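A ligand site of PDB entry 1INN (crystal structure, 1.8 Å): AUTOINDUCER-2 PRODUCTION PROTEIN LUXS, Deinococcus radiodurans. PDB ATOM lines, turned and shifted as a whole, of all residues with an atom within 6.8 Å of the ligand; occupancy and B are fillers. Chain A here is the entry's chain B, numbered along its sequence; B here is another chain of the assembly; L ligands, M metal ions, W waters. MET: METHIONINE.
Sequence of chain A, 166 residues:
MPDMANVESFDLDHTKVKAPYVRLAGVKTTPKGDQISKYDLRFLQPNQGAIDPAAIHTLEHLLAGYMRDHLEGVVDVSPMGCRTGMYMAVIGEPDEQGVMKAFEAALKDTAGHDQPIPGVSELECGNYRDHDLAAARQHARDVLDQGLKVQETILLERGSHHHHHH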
ATOM      1  N   HIS A  57      19.625 -20.766  33.379  1.00  0.00           N
ATOM      2  CA  HIS A  57      19.950 -20.622  31.962  1.00  0.00           C
ATOM      3  C   HIS A  57      19.488 -19.213  31.510  1.00  0.00           C
ATOM      4  O   HIS A  57      20.207 -18.522  30.795  1.00  0.00           O
ATOM      5  CB  HIS A  57      19.222 -21.706  31.159  1.00  0.00           C
ATOM      6  CG  HIS A  57      19.559 -21.745  29.701  1.00  0.00           C
ATOM      7  ND1 HIS A  57      18.809 -22.446  28.788  1.00  0.00           N
ATOM      8  CD2 HIS A  57      20.577 -21.187  28.993  1.00  0.00           C
ATOM      9  CE1 HIS A  57      19.334 -22.324  27.581  1.00  0.00           C
ATOM     10  NE2 HIS A  57      20.412 -21.562  27.682  1.00  0.00           N
ATOM     11  N   GLU A  60      21.775 -16.541  32.886  1.00  0.00           N
ATOM     12  CA  GLU A  60      23.023 -16.497  32.128  1.00  0.00           C
ATOM     13  C   GLU A  60      22.809 -15.625  30.879  1.00  0.00           C
ATOM     14  O   GLU A  60      23.606 -14.727  30.629  1.00  0.00           O
ATOM     15  CB  GLU A  60      23.414 -17.924  31.746  1.00  0.00           C
ATOM     16  CG  GLU A  60      24.653 -18.083  30.897  1.00  0.00           C
ATOM     17  CD  GLU A  60      24.666 -19.445  30.201  1.00  0.00           C
ATOM     18  OE1 GLU A  60      23.638 -19.811  29.575  1.00  0.00           O
ATOM     19  OE2 GLU A  60      25.684 -20.165  30.261  1.00  0.00           O
ATOM     20  N   HIS A  61      21.733 -15.848  30.122  1.00  0.00           N
ATOM     21  CA  HIS A  61      21.484 -15.026  28.941  1.00  0.00           C
ATOM     22  C   HIS A  61      21.383 -13.528  29.293  1.00  0.00           C
ATOM     23  O   HIS A  61      21.966 -12.689  28.620  1.00  0.00           O
ATOM     24  CB  HIS A  61      20.182 -15.440  28.234  1.00  0.00           C
ATOM     25  CG  HIS A  61      20.329 -16.636  27.339  1.00  0.00           C
ATOM     26  ND1 HIS A  61      19.894 -16.634  26.032  1.00  0.00           N
ATOM     27  CD2 HIS A  61      20.875 -17.858  27.568  1.00  0.00           C
ATOM     28  CE1 HIS A  61      20.168 -17.814  25.493  1.00  0.00           C
ATOM     29  NE2 HIS A  61      20.754 -18.571  26.399  1.00  0.00           N
ATOM     30  N   LEU A  62      20.620 -13.209  30.347  1.00  0.00           N
ATOM     31  CA  LEU A  62      20.439 -11.814  30.740  1.00  0.00           C
ATOM     32  C   LEU A  62      21.690 -11.148  31.319  1.00  0.00           C
ATOM     33  O   LEU A  62      22.055 -10.037  30.928  1.00  0.00           O
ATOM     34  CB  LEU A  62      19.285 -11.718  31.753  1.00  0.00           C
ATOM     35  CG  LEU A  62      17.909 -12.103  31.197  1.00  0.00           C
ATOM     36  CD1 LEU A  62      16.883 -12.137  32.324  1.00  0.00           C
ATOM     37  CD2 LEU A  62      17.486 -11.090  30.139  1.00  0.00           C
ATOM     38  N   ALA A  64      24.790 -12.079  30.932  1.00  0.00           N
ATOM     39  CA  ALA A  64      25.891 -12.029  29.977  1.00  0.00           C
ATOM     40  C   ALA A  64      25.894 -10.627  29.363  1.00  0.00           C
ATOM     41  O   ALA A  64      26.952 -10.022  29.167  1.00  0.00           O
ATOM     42  CB  ALA A  64      25.706 -13.063  28.883  1.00  0.00           C
ATOM     43  N   GLY A  65      24.698 -10.133  29.061  1.00  0.00           N
ATOM     44  CA  GLY A  65      24.595  -8.811  28.485  1.00  0.00           C
ATOM     45  C   GLY A  65      24.662  -7.683  29.521  1.00  0.00           C
ATOM     46  O   GLY A  65      25.464  -6.759  29.386  1.00  0.00           O
ATOM     47  N   ARG A  68      28.048  -6.937  31.197  1.00  0.00           N
ATOM     48  CA  ARG A  68      28.924  -6.248  30.264  1.00  0.00           C
ATOM     49  C   ARG A  68      28.533  -4.786  30.060  1.00  0.00           C
ATOM     50  O   ARG A  68      29.365  -3.976  29.677  1.00  0.00           O
ATOM     51  CB  ARG A  68      29.005  -7.012  28.932  1.00  0.00           C
ATOM     52  CG  ARG A  68      29.651  -8.425  29.091  1.00  0.00           C
ATOM     53  CD  ARG A  68      29.983  -9.062  27.740  1.00  0.00           C
ATOM     54  NE  ARG A  68      30.866 -10.224  27.814  1.00  0.00           N
ATOM     55  CZ  ARG A  68      30.503 -11.449  28.178  1.00  0.00           C
ATOM     56  NH1 ARG A  68      31.404 -12.447  28.192  1.00  0.00           N
ATOM     57  NH2 ARG A  68      29.247 -11.703  28.523  1.00  0.00           N
ATOM     58  N   VAL A  74      35.076  -8.100  30.892  1.00  0.00           N
ATOM     59  CA  VAL A  74      34.476  -9.395  31.233  1.00  0.00           C
ATOM     60  C   VAL A  74      34.888 -10.468  30.224  1.00  0.00           C
ATOM     61  O   VAL A  74      34.739 -10.289  29.011  1.00  0.00           O
ATOM     62  CB  VAL A  74      32.928  -9.286  31.266  1.00  0.00           C
ATOM     63  CG1 VAL A  74      32.295 -10.653  31.533  1.00  0.00           C
ATOM     64  CG2 VAL A  74      32.519  -8.290  32.341  1.00  0.00           C
ATOM     65  N   VAL A  75      35.446 -11.560  30.725  1.00  0.00           N
ATOM     66  CA  VAL A  75      35.877 -12.650  29.854  1.00  0.00           C
ATOM     67  C   VAL A  75      34.793 -13.705  29.709  1.00  0.00           C
ATOM     68  O   VAL A  75      34.628 -14.290  28.642  1.00  0.00           O
ATOM     69  CB  VAL A  75      37.142 -13.312  30.394  1.00  0.00           C
ATOM     70  CG1 VAL A  75      37.477 -14.564  29.582  1.00  0.00           C
ATOM     71  CG2 VAL A  75      38.281 -12.328  30.341  1.00  0.00           C
ATOM     72  N   ASP A  76      34.052 -13.918  30.788  1.00  0.00           N
ATOM     73  CA  ASP A  76      32.999 -14.914  30.789  1.00  0.00           C
ATOM     74  C   ASP A  76      32.108 -14.724  32.006  1.00  0.00           C
ATOM     75  O   ASP A  76      32.573 -14.330  33.080  1.00  0.00           O
ATOM     76  CB  ASP A  76      33.610 -16.318  30.832  1.00  0.00           C
ATOM     77  CG  ASP A  76      32.577 -17.422  30.667  1.00  0.00           C
ATOM     78  OD1 ASP A  76      32.113 -17.619  29.528  1.00  0.00           O
ATOM     79  OD2 ASP A  76      32.212 -18.084  31.674  1.00  0.00           O
ATOM     80  N   VAL A  77      30.829 -15.004  31.834  1.00  0.00           N
ATOM     81  CA  VAL A  77      29.837 -14.945  32.903  1.00  0.00           C
ATOM     82  C   VAL A  77      29.129 -16.267  32.724  1.00  0.00           C
ATOM     83  O   VAL A  77      28.469 -16.474  31.712  1.00  0.00           O
ATOM     84  CB  VAL A  77      28.826 -13.811  32.690  1.00  0.00           C
ATOM     85  CG1 VAL A  77      27.758 -13.861  33.792  1.00  0.00           C
ATOM     86  CG2 VAL A  77      29.523 -12.490  32.721  1.00  0.00           C
ATOM     87  N   SER A  78      29.271 -17.181  33.689  1.00  0.00           N
ATOM     88  CA  SER A  78      28.646 -18.493  33.545  1.00  0.00           C
ATOM     89  C   SER A  78      28.017 -19.015  34.833  1.00  0.00           C
ATOM     90  O   SER A  78      28.394 -18.604  35.929  1.00  0.00           O
ATOM     91  CB  SER A  78      29.683 -19.534  33.096  1.00  0.00           C
ATOM     92  OG  SER A  78      30.054 -19.400  31.738  1.00  0.00           O
ATOM     93  N   PRO A  79      27.052 -19.921  34.716  1.00  0.00           N
ATOM     94  CA  PRO A  79      26.424 -20.459  35.924  1.00  0.00           C
ATOM     95  C   PRO A  79      27.389 -21.421  36.600  1.00  0.00           C
ATOM     96  O   PRO A  79      28.259 -22.006  35.947  1.00  0.00           O
ATOM     97  CB  PRO A  79      25.204 -21.191  35.390  1.00  0.00           C
ATOM     98  CG  PRO A  79      25.604 -21.597  34.012  1.00  0.00           C
ATOM     99  CD  PRO A  79      26.363 -20.392  33.500  1.00  0.00           C
ATOM    100  N   GLU A 124      20.604 -19.333  18.020  1.00  0.00           N
ATOM    101  CA  GLU A 124      21.510 -18.676  18.977  1.00  0.00           C
ATOM    102  C   GLU A 124      21.719 -19.343  20.322  1.00  0.00           C
ATOM    103  O   GLU A 124      22.582 -18.898  21.083  1.00  0.00           O
ATOM    104  CB  GLU A 124      21.004 -17.252  19.261  1.00  0.00           C
ATOM    105  CG  GLU A 124      20.662 -16.437  18.011  1.00  0.00           C
ATOM    106  CD  GLU A 124      19.738 -15.255  18.333  1.00  0.00           C
ATOM    107  OE1 GLU A 124      18.575 -15.485  18.735  1.00  0.00           O
ATOM    108  OE2 GLU A 124      20.184 -14.096  18.199  1.00  0.00           O
ATOM    109  N   CYS A 125      20.950 -20.381  20.614  1.00  0.00           N
ATOM    110  CA  CYS A 125      21.023 -21.041  21.910  1.00  0.00           C
ATOM    111  C   CYS A 125      21.026 -22.563  21.810  1.00  0.00           C
ATOM    112  O   CYS A 125      20.312 -23.143  20.993  1.00  0.00           O
ATOM    113  CB  CYS A 125      19.829 -20.544  22.729  1.00  0.00           C
ATOM    114  SG  CYS A 125      19.484 -21.372  24.287  1.00  0.00           S
ATOM    115  N   VAL B   7      26.435 -10.025  23.019  1.00  0.00           N
ATOM    116  CA  VAL B   7      26.982 -11.236  23.593  1.00  0.00           C
ATOM    117  C   VAL B   7      27.414 -12.103  22.406  1.00  0.00           C
ATOM    118  O   VAL B   7      26.581 -12.576  21.639  1.00  0.00           O
ATOM    119  CB  VAL B   7      25.901 -11.940  24.443  1.00  0.00           C
ATOM    120  CG1 VAL B   7      26.460 -13.213  25.051  1.00  0.00           C
ATOM    121  CG2 VAL B   7      25.398 -10.972  25.527  1.00  0.00           C
ATOM    122  N   GLU B   8      28.735 -12.272  22.257  1.00  0.00           N
ATOM    123  CA  GLU B   8      29.319 -13.044  21.163  1.00  0.00           C
ATOM    124  C   GLU B   8      28.717 -14.450  21.041  1.00  0.00           C
ATOM    125  O   GLU B   8      28.595 -14.966  19.937  1.00  0.00           O
ATOM    126  CB  GLU B   8      30.844 -13.183  21.359  1.00  0.00           C
ATOM    127  CG  GLU B   8      31.594 -11.883  21.615  1.00  0.00           C
ATOM    128  CD  GLU B   8      33.035 -12.125  22.072  1.00  0.00           C
ATOM    129  OE1 GLU B   8      33.618 -11.228  22.730  1.00  0.00           O
ATOM    130  OE2 GLU B   8      33.602 -13.203  21.772  1.00  0.00           O
ATOM    131  N   SER B   9      28.351 -15.058  22.169  1.00  0.00           N
ATOM    132  CA  SER B   9      27.778 -16.404  22.140  1.00  0.00           C
ATOM    133  C   SER B   9      26.594 -16.560  21.191  1.00  0.00           C
ATOM    134  O   SER B   9      26.462 -17.586  20.511  1.00  0.00           O
ATOM    135  CB  SER B   9      27.361 -16.820  23.558  1.00  0.00           C
ATOM    136  OG  SER B   9      28.488 -16.764  24.425  1.00  0.00           O
ATOM    137  N   PHE B  10      25.737 -15.534  21.128  1.00  0.00           N
ATOM    138  CA  PHE B  10      24.558 -15.561  20.267  1.00  0.00           C
ATOM    139  C   PHE B  10      24.844 -15.487  18.760  1.00  0.00           C
ATOM    140  O   PHE B  10      23.950 -15.702  17.948  1.00  0.00           O
ATOM    141  CB  PHE B  10      23.622 -14.397  20.633  1.00  0.00           C
ATOM    142  CG  PHE B  10      23.170 -14.395  22.070  1.00  0.00           C
ATOM    143  CD1 PHE B  10      22.779 -13.208  22.688  1.00  0.00           C
ATOM    144  CD2 PHE B  10      23.134 -15.576  22.820  1.00  0.00           C
ATOM    145  CE1 PHE B  10      22.363 -13.201  24.022  1.00  0.00           C
ATOM    146  CE2 PHE B  10      22.723 -15.566  24.142  1.00  0.00           C
ATOM    147  CZ  PHE B  10      22.340 -14.389  24.745  1.00  0.00           C
ATOM    148  N   LYS B  38      39.148 -18.365  24.685  1.00  0.00           N
ATOM    149  CA  LYS B  38      38.000 -19.039  25.285  1.00  0.00           C
ATOM    150  C   LYS B  38      37.584 -20.120  24.313  1.00  0.00           C
ATOM    151  O   LYS B  38      37.456 -19.871  23.117  1.00  0.00           O
ATOM    152  CB  LYS B  38      36.847 -18.042  25.482  1.00  0.00           C
ATOM    153  CG  LYS B  38      37.122 -17.004  26.567  1.00  0.00           C
ATOM    154  CD  LYS B  38      36.614 -15.597  26.183  1.00  0.00           C
ATOM    155  CE  LYS B  38      35.106 -15.530  26.042  1.00  0.00           C
ATOM    156  NZ  LYS B  38      34.670 -14.144  25.684  1.00  0.00           N
ATOM    157  N   PRO B  79      30.367 -24.896  33.280  1.00  0.00           N
ATOM    158  CA  PRO B  79      29.315 -25.544  32.477  1.00  0.00           C
ATOM    159  C   PRO B  79      28.497 -24.462  31.771  1.00  0.00           C
ATOM    160  O   PRO B  79      28.375 -23.333  32.253  1.00  0.00           O
ATOM    161  CB  PRO B  79      28.492 -26.275  33.530  1.00  0.00           C
ATOM    162  CG  PRO B  79      28.596 -25.358  34.738  1.00  0.00           C
ATOM    163  CD  PRO B  79      30.070 -24.955  34.719  1.00  0.00           C
ATOM    164  N   MET B  80      27.941 -24.784  30.603  1.00  0.00           N
ATOM    165  CA  MET B  80      27.095 -23.812  29.891  1.00  0.00           C
ATOM    166  C   MET B  80      25.679 -23.912  30.430  1.00  0.00           C
ATOM    167  O   MET B  80      25.254 -24.993  30.849  1.00  0.00           O
ATOM    168  CB  MET B  80      27.064 -24.134  28.391  1.00  0.00           C
ATOM    169  CG  MET B  80      28.400 -24.111  27.732  1.00  0.00           C
ATOM    170  SD  MET B  80      28.209 -24.418  25.828  1.00  0.00           S
ATOM    171  CE  MET B  80      27.232 -26.014  25.808  1.00  0.00           C
ATOM    172  N   GLY B  81      24.944 -22.806  30.403  1.00  0.00           N
ATOM    173  CA  GLY B  81      23.564 -22.830  30.858  1.00  0.00           C
ATOM    174  C   GLY B  81      22.716 -23.760  29.995  1.00  0.00           C
ATOM    175  O   GLY B  81      21.750 -24.359  30.496  1.00  0.00           O
ATOM    176  N   CYS B  82      23.074 -23.897  28.716  1.00  0.00           N
ATOM    177  CA  CYS B  82      22.334 -24.777  27.823  1.00  0.00           C
ATOM    178  C   CYS B  82      22.645 -26.255  28.074  1.00  0.00           C
ATOM    179  O   CYS B  82      22.008 -27.143  27.500  1.00  0.00           O
ATOM    180  CB  CYS B  82      22.623 -24.397  26.363  1.00  0.00           C
ATOM    181  SG  CYS B  82      24.376 -24.351  25.916  1.00  0.00           S
ATOM    182  N   TYR B  87      32.567 -24.140  28.847  1.00  0.00           N
ATOM    183  CA  TYR B  87      33.374 -23.055  28.335  1.00  0.00           C
ATOM    184  C   TYR B  87      34.668 -23.105  29.137  1.00  0.00           C
ATOM    185  O   TYR B  87      34.652 -23.366  30.346  1.00  0.00           O
ATOM    186  CB  TYR B  87      32.714 -21.691  28.540  1.00  0.00           C
ATOM    187  CG  TYR B  87      31.935 -21.173  27.354  1.00  0.00           C
ATOM    188  CD1 TYR B  87      32.553 -21.039  26.095  1.00  0.00           C
ATOM    189  CD2 TYR B  87      30.600 -20.804  27.480  1.00  0.00           C
ATOM    190  CE1 TYR B  87      31.835 -20.540  24.992  1.00  0.00           C
ATOM    191  CE2 TYR B  87      29.869 -20.301  26.381  1.00  0.00           C
ATOM    192  CZ  TYR B  87      30.501 -20.175  25.148  1.00  0.00           C
ATOM    193  OH  TYR B  87      29.799 -19.646  24.072  1.00  0.00           O
HETATM  194  N   MET L   1      29.387 -17.624  29.371  1.00  0.00           N
HETATM  195  CA  MET L   1      28.788 -16.797  28.281  1.00  0.00           C
HETATM  196  C   MET L   1      29.362 -15.375  28.260  1.00  0.00           C
HETATM  197  O   MET L   1      30.390 -15.144  28.936  1.00  0.00           O
HETATM  198  CB  MET L   1      27.269 -16.737  28.440  1.00  0.00           C
HETATM  199  CG  MET L   1      26.552 -16.087  27.275  1.00  0.00           C
HETATM  200  SD  MET L   1      24.788 -16.397  27.318  1.00  0.00           S
HETATM  201  CE  MET L   1      24.749 -18.036  26.544  1.00  0.00           C
HETATM  202  OXT MET L   1      28.794 -14.506  27.563  1.00  0.00           O
HETATM  203 ZN    ZN M   1      21.010 -20.569  25.870  1.00  0.00          ZN
HETATM  204  O   HOH W   1      29.457 -14.125  24.964  1.00  0.00           O
HETATM  205  O   HOH W   2      28.142 -20.201  29.159  1.00  0.00           O
HETATM  206  O   HOH W   3      26.699 -20.886  26.953  1.00  0.00           O
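Glu 60 touches the ligand (OE1 to CE, 3.7 Å).
His 61 touches the ligand.
CB of Ala 64 touches CG of the ligand, 3.5 Å away.
CG1 of Val 7 of chain B touches CG of the ligand (3.6 Å).
Ser 9 of chain B touches the ligand.
CE2 of Phe 10 of chain B touches SD of the ligand (3.9 Å).
Tyr 87 of chain B touches the ligand.
Hydrophobic or aromatic side chains that line the ligand: Ala 64, Val 7 of chain B, Phe 10 of chain B and Tyr 87 of chain B.
Within 4 Å of the ligand: Glu 60, His 61, Ala 64, Arg 68, Asp 76, Val 77, Ser 78, Val 7 of chain B, Ser 9 of chain B, Phe 10 of chain B and Tyr 87 of chain B.
Along chain A the residues within 4 Å of the ligand span positions 60 to 78.
N of the ligand is in salt-bridge range of OD1 of Asp 76.
N of Val 77 lies within hydrogen-bond range of O of the ligand.
The backbone carbonyl oxygen of Val 77 sits at hydrogen-bond distance from a nitrogen (N) of the ligand (2.8 Å).
The guanidinium group (NH1) of Arg 68 is in salt-bridge range of an oxygen (O) of the ligand, at 3.0 Å.
OG of Ser 78 is in hydrogen-bond range of N of the ligand (3.0 Å).
Water W1 lies within hydrogen-bond range of an oxygen (OXT) of the ligand (2.7 Å), the side-chain hydroxyl (OG) of Ser 9 of chain B (2.9 Å) and the backbone NH (N) of Glu 8 of chain B (3.4 Å).
Water W2 lies within hydrogen-bond range of OE2 of Glu 60, N of the ligand and OG of Ser 78.
OD2 of Asp 76 is in hydrogen-bond range of OG of Ser 78.
The backbone carbonyl oxygen (O) of Ala 64 lies within hydrogen-bond range of the guanidinium group (NH2) of Arg 68, at 2.9 Å.
The side-chain hydroxyl (OH) of Tyr 87 of chain B is in hydrogen-bond range of the side-chain hydroxyl (OG) of Ser 9 of chain B (3.2 Å).
N of Gly 81 of chain B is in hydrogen-bond range of OE2 of Glu 60 (2.7 Å).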
